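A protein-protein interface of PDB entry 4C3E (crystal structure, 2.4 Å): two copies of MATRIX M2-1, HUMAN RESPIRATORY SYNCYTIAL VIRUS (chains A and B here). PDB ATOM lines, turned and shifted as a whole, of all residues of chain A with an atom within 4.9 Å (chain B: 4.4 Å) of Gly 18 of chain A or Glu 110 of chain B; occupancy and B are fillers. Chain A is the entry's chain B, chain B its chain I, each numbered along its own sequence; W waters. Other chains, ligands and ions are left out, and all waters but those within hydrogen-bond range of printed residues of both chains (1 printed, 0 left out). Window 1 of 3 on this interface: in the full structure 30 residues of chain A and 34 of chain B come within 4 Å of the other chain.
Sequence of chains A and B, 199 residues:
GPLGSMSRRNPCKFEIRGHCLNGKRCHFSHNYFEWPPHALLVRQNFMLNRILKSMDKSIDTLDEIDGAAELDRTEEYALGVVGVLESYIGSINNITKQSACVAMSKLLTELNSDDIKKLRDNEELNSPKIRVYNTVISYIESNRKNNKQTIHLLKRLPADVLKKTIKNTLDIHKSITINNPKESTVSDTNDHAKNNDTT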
ATOM      1  N   PHE A  14      12.051 -11.824   3.071  1.00  0.00           N
ATOM      2  CA  PHE A  14      12.794 -10.897   3.920  1.00  0.00           C
ATOM      3  C   PHE A  14      12.130  -9.506   3.890  1.00  0.00           C
ATOM      4  O   PHE A  14      12.226  -8.755   4.863  1.00  0.00           O
ATOM      5  CB  PHE A  14      14.267 -10.785   3.512  1.00  0.00           C
ATOM      6  CG  PHE A  14      15.031 -12.048   3.731  1.00  0.00           C
ATOM      7  CD1 PHE A  14      15.591 -12.326   4.972  1.00  0.00           C
ATOM      8  CD2 PHE A  14      15.164 -12.989   2.720  1.00  0.00           C
ATOM      9  CE1 PHE A  14      16.278 -13.501   5.179  1.00  0.00           C
ATOM     10  CE2 PHE A  14      15.855 -14.183   2.927  1.00  0.00           C
ATOM     11  CZ  PHE A  14      16.419 -14.433   4.156  1.00  0.00           C
ATOM     12  N   GLU A  15      11.562  -9.153   2.749  1.00  0.00           N
ATOM     13  CA  GLU A  15      11.070  -7.804   2.495  1.00  0.00           C
ATOM     14  C   GLU A  15       9.732  -7.757   3.215  1.00  0.00           C
ATOM     15  O   GLU A  15       9.417  -6.787   3.853  1.00  0.00           O
ATOM     16  CB  GLU A  15      10.897  -7.557   0.989  1.00  0.00           C
ATOM     17  CG  GLU A  15      10.455  -6.151   0.558  1.00  0.00           C
ATOM     18  CD  GLU A  15      11.474  -5.110   0.802  1.00  0.00           C
ATOM     19  OE1 GLU A  15      12.652  -5.456   0.959  1.00  0.00           O
ATOM     20  OE2 GLU A  15      11.110  -3.898   0.863  1.00  0.00           O
ATOM     21  N   ILE A  16       9.012  -8.858   3.179  1.00  0.00           N
ATOM     22  CA  ILE A  16       7.799  -8.979   3.963  1.00  0.00           C
ATOM     23  C   ILE A  16       7.990  -8.657   5.426  1.00  0.00           C
ATOM     24  O   ILE A  16       7.110  -8.097   6.023  1.00  0.00           O
ATOM     25  CB  ILE A  16       7.140 -10.346   3.805  1.00  0.00           C
ATOM     26  CG1 ILE A  16       6.663 -10.530   2.374  1.00  0.00           C
ATOM     27  CG2 ILE A  16       5.917 -10.417   4.704  1.00  0.00           C
ATOM     28  CD1 ILE A  16       6.096 -11.906   2.076  1.00  0.00           C
ATOM     29  N   ARG A  17       9.119  -8.997   6.014  1.00  0.00           N
ATOM     30  CA  ARG A  17       9.401  -8.655   7.433  1.00  0.00           C
ATOM     31  C   ARG A  17      10.151  -7.414   7.615  1.00  0.00           C
ATOM     32  O   ARG A  17      10.500  -7.083   8.732  1.00  0.00           O
ATOM     33  CB  ARG A  17      10.296  -9.682   8.067  1.00  0.00           C
ATOM     34  CG  ARG A  17       9.705 -11.035   8.070  1.00  0.00           C
ATOM     35  CD  ARG A  17      10.700 -12.043   8.606  1.00  0.00           C
ATOM     36  NE  ARG A  17       9.894 -13.159   8.998  1.00  0.00           N
ATOM     37  CZ  ARG A  17       9.426 -13.333  10.231  1.00  0.00           C
ATOM     38  NH1 ARG A  17       9.786 -12.500  11.223  1.00  0.00           N
ATOM     39  NH2 ARG A  17       8.628 -14.367  10.438  1.00  0.00           N
ATOM     40  N   GLY A  18      10.469  -6.696   6.550  1.00  0.00           N
ATOM     41  CA  GLY A  18      11.154  -5.372   6.733  1.00  0.00           C
ATOM     42  C   GLY A  18      11.775  -4.993   5.408  1.00  0.00           C
ATOM     43  O   GLY A  18      11.065  -4.825   4.412  1.00  0.00           O
ATOM     44  N   HIS A  19      13.100  -5.072   5.379  1.00  0.00           N
ATOM     45  CA  HIS A  19      13.922  -4.747   4.204  1.00  0.00           C
ATOM     46  C   HIS A  19      14.859  -5.914   3.859  1.00  0.00           C
ATOM     47  O   HIS A  19      15.633  -6.355   4.693  1.00  0.00           O
ATOM     48  CB  HIS A  19      14.722  -3.543   4.573  1.00  0.00           C
ATOM     49  CG  HIS A  19      13.888  -2.325   4.768  1.00  0.00           C
ATOM     50  ND1 HIS A  19      13.096  -1.793   3.764  1.00  0.00           N
ATOM     51  CD2 HIS A  19      13.735  -1.505   5.838  1.00  0.00           C
ATOM     52  CE1 HIS A  19      12.497  -0.703   4.211  1.00  0.00           C
ATOM     53  NE2 HIS A  19      12.879  -0.497   5.459  1.00  0.00           N
ATOM     54  N   CYS A  20      14.744  -6.440   2.645  1.00  0.00           N
ATOM     55  CA  CYS A  20      15.664  -7.444   2.125  1.00  0.00           C
ATOM     56  C   CYS A  20      17.023  -6.861   2.129  1.00  0.00           C
ATOM     57  O   CYS A  20      17.204  -5.741   1.720  1.00  0.00           O
ATOM     58  CB  CYS A  20      15.306  -7.841   0.738  1.00  0.00           C
ATOM     59  SG  CYS A  20      16.283  -9.215   0.102  1.00  0.00           S
ATOM     60  N   LEU A  21      17.987  -7.590   2.685  1.00  0.00           N
ATOM     61  CA  LEU A  21      19.380  -7.104   2.786  1.00  0.00           C
ATOM     62  C   LEU A  21      20.344  -7.882   1.869  1.00  0.00           C
ATOM     63  O   LEU A  21      21.535  -7.775   1.975  1.00  0.00           O
ATOM     64  CB  LEU A  21      19.843  -7.267   4.213  1.00  0.00           C
ATOM     65  CG  LEU A  21      19.233  -6.387   5.296  1.00  0.00           C
ATOM     66  CD1 LEU A  21      19.810  -6.851   6.624  1.00  0.00           C
ATOM     67  CD2 LEU A  21      19.485  -4.907   5.115  1.00  0.00           C
ATOM     68  N   ARG A  43       3.274  -7.307   5.682  1.00  0.00           N
ATOM     69  CA  ARG A  43       4.451  -6.464   5.862  1.00  0.00           C
ATOM     70  C   ARG A  43       4.135  -5.258   6.637  1.00  0.00           C
ATOM     71  O   ARG A  43       4.952  -4.742   7.411  1.00  0.00           O
ATOM     72  CB  ARG A  43       5.066  -6.091   4.477  1.00  0.00           C
ATOM     73  CG  ARG A  43       6.285  -5.182   4.547  1.00  0.00           C
ATOM     74  CD  ARG A  43       6.909  -4.933   3.168  1.00  0.00           C
ATOM     75  NE  ARG A  43       8.173  -4.217   3.375  1.00  0.00           N
ATOM     76  CZ  ARG A  43       8.290  -2.913   3.505  1.00  0.00           C
ATOM     77  NH1 ARG A  43       7.289  -2.098   3.275  1.00  0.00           N
ATOM     78  NH2 ARG A  43       9.469  -2.417   3.778  1.00  0.00           N
ATOM     79  N   MET A  47       6.135  -3.916   9.830  1.00  0.00           N
ATOM     80  CA  MET A  47       6.763  -2.574   9.801  1.00  0.00           C
ATOM     81  C   MET A  47       6.179  -1.697  10.931  1.00  0.00           C
ATOM     82  O   MET A  47       6.892  -0.900  11.574  1.00  0.00           O
ATOM     83  CB  MET A  47       6.573  -1.915   8.421  1.00  0.00           C
ATOM     84  CG  MET A  47       7.425  -2.474   7.279  1.00  0.00           C
ATOM     85  SD  MET A  47       9.158  -2.062   7.514  1.00  0.00           S
ATOM     86  CE  MET A  47       9.154  -0.318   7.242  1.00  0.00           C
ATOM     87  N   ARG A  50       7.859  -2.467  14.019  1.00  0.00           N
ATOM     88  CA  ARG A  50       9.204  -1.886  14.067  1.00  0.00           C
ATOM     89  C   ARG A  50       9.185  -0.411  14.317  1.00  0.00           C
ATOM     90  O   ARG A  50       9.959   0.118  15.093  1.00  0.00           O
ATOM     91  CB  ARG A  50       9.887  -2.200  12.763  1.00  0.00           C
ATOM     92  CG  ARG A  50      11.378  -2.073  12.855  1.00  0.00           C
ATOM     93  CD  ARG A  50      12.066  -2.800  11.716  1.00  0.00           C
ATOM     94  NE  ARG A  50      13.287  -2.062  11.378  1.00  0.00           N
ATOM     95  CZ  ARG A  50      14.013  -2.321  10.294  1.00  0.00           C
ATOM     96  NH1 ARG A  50      13.636  -3.306   9.490  1.00  0.00           N
ATOM     97  NH2 ARG A  50      15.089  -1.589  10.018  1.00  0.00           N
ATOM     98  N   LYS B 106      23.990  -2.719  10.396  1.00  0.00           N
ATOM     99  CA  LYS B 106      22.763  -2.670   9.619  1.00  0.00           C
ATOM    100  C   LYS B 106      21.995  -3.941   9.727  1.00  0.00           C
ATOM    101  O   LYS B 106      20.777  -3.929   9.686  1.00  0.00           O
ATOM    102  CB  LYS B 106      23.052  -2.369   8.150  1.00  0.00           C
ATOM    103  CG  LYS B 106      23.719  -1.030   7.955  1.00  0.00           C
ATOM    104  CD  LYS B 106      23.075  -0.244   6.847  1.00  0.00           C
ATOM    105  CE  LYS B 106      23.898  -0.189   5.575  1.00  0.00           C
ATOM    106  NZ  LYS B 106      24.852   0.924   5.703  1.00  0.00           N
ATOM    107  N   LEU B 107      22.690  -5.063   9.795  1.00  0.00           N
ATOM    108  CA  LEU B 107      22.012  -6.357   9.922  1.00  0.00           C
ATOM    109  C   LEU B 107      21.281  -6.461  11.286  1.00  0.00           C
ATOM    110  O   LEU B 107      20.200  -7.009  11.364  1.00  0.00           O
ATOM    111  CB  LEU B 107      23.014  -7.526   9.818  1.00  0.00           C
ATOM    112  CG  LEU B 107      22.457  -8.917  10.023  1.00  0.00           C
ATOM    113  CD1 LEU B 107      21.409  -9.224   9.004  1.00  0.00           C
ATOM    114  CD2 LEU B 107      23.579  -9.925   9.859  1.00  0.00           C
ATOM    115  N   LEU B 108      21.936  -5.991  12.325  1.00  0.00           N
ATOM    116  CA  LEU B 108      21.422  -6.048  13.668  1.00  0.00           C
ATOM    117  C   LEU B 108      20.128  -5.195  13.751  1.00  0.00           C
ATOM    118  O   LEU B 108      19.115  -5.681  14.239  1.00  0.00           O
ATOM    119  CB  LEU B 108      22.476  -5.572  14.668  1.00  0.00           C
ATOM    120  CG  LEU B 108      23.646  -6.528  14.862  1.00  0.00           C
ATOM    121  CD1 LEU B 108      24.775  -5.831  15.646  1.00  0.00           C
ATOM    122  CD2 LEU B 108      23.235  -7.797  15.554  1.00  0.00           C
ATOM    123  N   THR B 109      20.183  -3.965  13.213  1.00  0.00           N
ATOM    124  CA  THR B 109      19.017  -3.077  13.042  1.00  0.00           C
ATOM    125  C   THR B 109      17.867  -3.761  12.361  1.00  0.00           C
ATOM    126  O   THR B 109      16.738  -3.565  12.742  1.00  0.00           O
ATOM    127  CB  THR B 109      19.378  -1.837  12.270  1.00  0.00           C
ATOM    128  OG1 THR B 109      20.291  -1.051  13.066  1.00  0.00           O
ATOM    129  CG2 THR B 109      18.150  -1.009  11.897  1.00  0.00           C
ATOM    130  N   GLU B 110      18.121  -4.672  11.459  1.00  0.00           N
ATOM    131  CA  GLU B 110      17.029  -5.361  10.787  1.00  0.00           C
ATOM    132  C   GLU B 110      16.456  -6.525  11.598  1.00  0.00           C
ATOM    133  O   GLU B 110      15.365  -7.065  11.316  1.00  0.00           O
ATOM    134  CB  GLU B 110      17.538  -5.871   9.433  1.00  0.00           C
ATOM    135  CG  GLU B 110      16.516  -6.636   8.621  1.00  0.00           C
ATOM    136  CD  GLU B 110      15.346  -5.775   8.153  1.00  0.00           C
ATOM    137  OE1 GLU B 110      15.518  -4.532   8.069  1.00  0.00           O
ATOM    138  OE2 GLU B 110      14.290  -6.368   7.747  1.00  0.00           O
ATOM    139  N   LEU B 111      17.200  -6.991  12.581  1.00  0.00           N
ATOM    140  CA  LEU B 111      16.705  -8.134  13.351  1.00  0.00           C
ATOM    141  C   LEU B 111      15.874  -7.620  14.498  1.00  0.00           C
ATOM    142  O   LEU B 111      16.114  -6.524  15.017  1.00  0.00           O
ATOM    143  CB  LEU B 111      17.877  -8.936  13.904  1.00  0.00           C
ATOM    144  CG  LEU B 111      18.690  -9.769  12.917  1.00  0.00           C
ATOM    145  CD1 LEU B 111      19.875 -10.382  13.633  1.00  0.00           C
ATOM    146  CD2 LEU B 111      17.834 -10.857  12.324  1.00  0.00           C
ATOM    147  N   ASN B 112      14.964  -8.424  15.002  1.00  0.00           N
ATOM    148  CA  ASN B 112      14.507  -8.100  16.347  1.00  0.00           C
ATOM    149  C   ASN B 112      14.618  -9.201  17.434  1.00  0.00           C
ATOM    150  O   ASN B 112      14.386 -10.399  17.200  1.00  0.00           O
ATOM    151  CB  ASN B 112      13.153  -7.430  16.300  1.00  0.00           C
ATOM    152  CG  ASN B 112      12.038  -8.394  16.370  1.00  0.00           C
ATOM    153  OD1 ASN B 112      11.361  -8.496  17.394  1.00  0.00           O
ATOM    154  ND2 ASN B 112      11.829  -9.119  15.298  1.00  0.00           N
HETATM  155  O   HOH W   1      13.734  -8.775   6.788  1.00  0.00           O
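Of the printed residues of chain B, Arg 17 of chain A touches Glu 110.
Of the printed residues of chain A, Leu 107 of chain B touches Leu 21 (3.7 Å).
Of the printed residues of chain B, Leu 21 of chain A touches Leu 107 (3.7 Å) and Glu 110 (3.7 Å).
Of the printed residues of chain B, His 19 of chain A touches Glu 110.
Of the printed residues of chain B, Arg 50 of chain A touches Thr 109 (3.6 Å) and Glu 110 (2.7 Å).
Printed residues of chain A that touch a printed residue of chain B: Arg 17, Gly 18, His 19, Leu 21 and Arg 50.
Hydrophobic or aromatic side chains of chain A that line the printed part of chain B: His 19 and Leu 21.
Along chain A the printed residues that touch a printed residue of chain B span positions 17 to 50.
Among the printed residues, Asp or Glu carboxylates within 4 Å of a Lys or Arg side-chain nitrogen of the other chain: Arg 50 of chain A with Glu 110 of chain B.
Among the printed residues, merely in contact across the chains: Gly 18 of chain A with Glu 110 of chain B, Arg 50 of chain A with Thr 109 of chain B, Leu 21 of chain A with Leu 107 of chain B, Leu 21 of chain A with Glu 110 of chain B and Arg 17 of chain A with Glu 110 of chain B.
O of Gly 18 of chain A sits at hydrogen-bond distance from NH2 of Arg 43 of chain A.
No position is printed for both chains.
Of the 7 pairs that touch across the chains among the printed residues, none has its exchanged pair printed and touching as well.
Water W1 bridges the backbone carbonyl oxygen of Phe 14 of chain A (2.4 Å) and the side-chain carboxylate of Glu 110 of chain B (2.6 Å).
The guanidinium group (NH1) of Arg 50 of chain A lies within salt-bridge range of the side-chain carboxylate (OE1) of Glu 110 of chain B, at 2.7 Å.
The side-chain carboxylate of Glu 110 of chain B sits at hydrogen-bond distance from the backbone NH of His 19 of chain A, at 3.0 Å.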
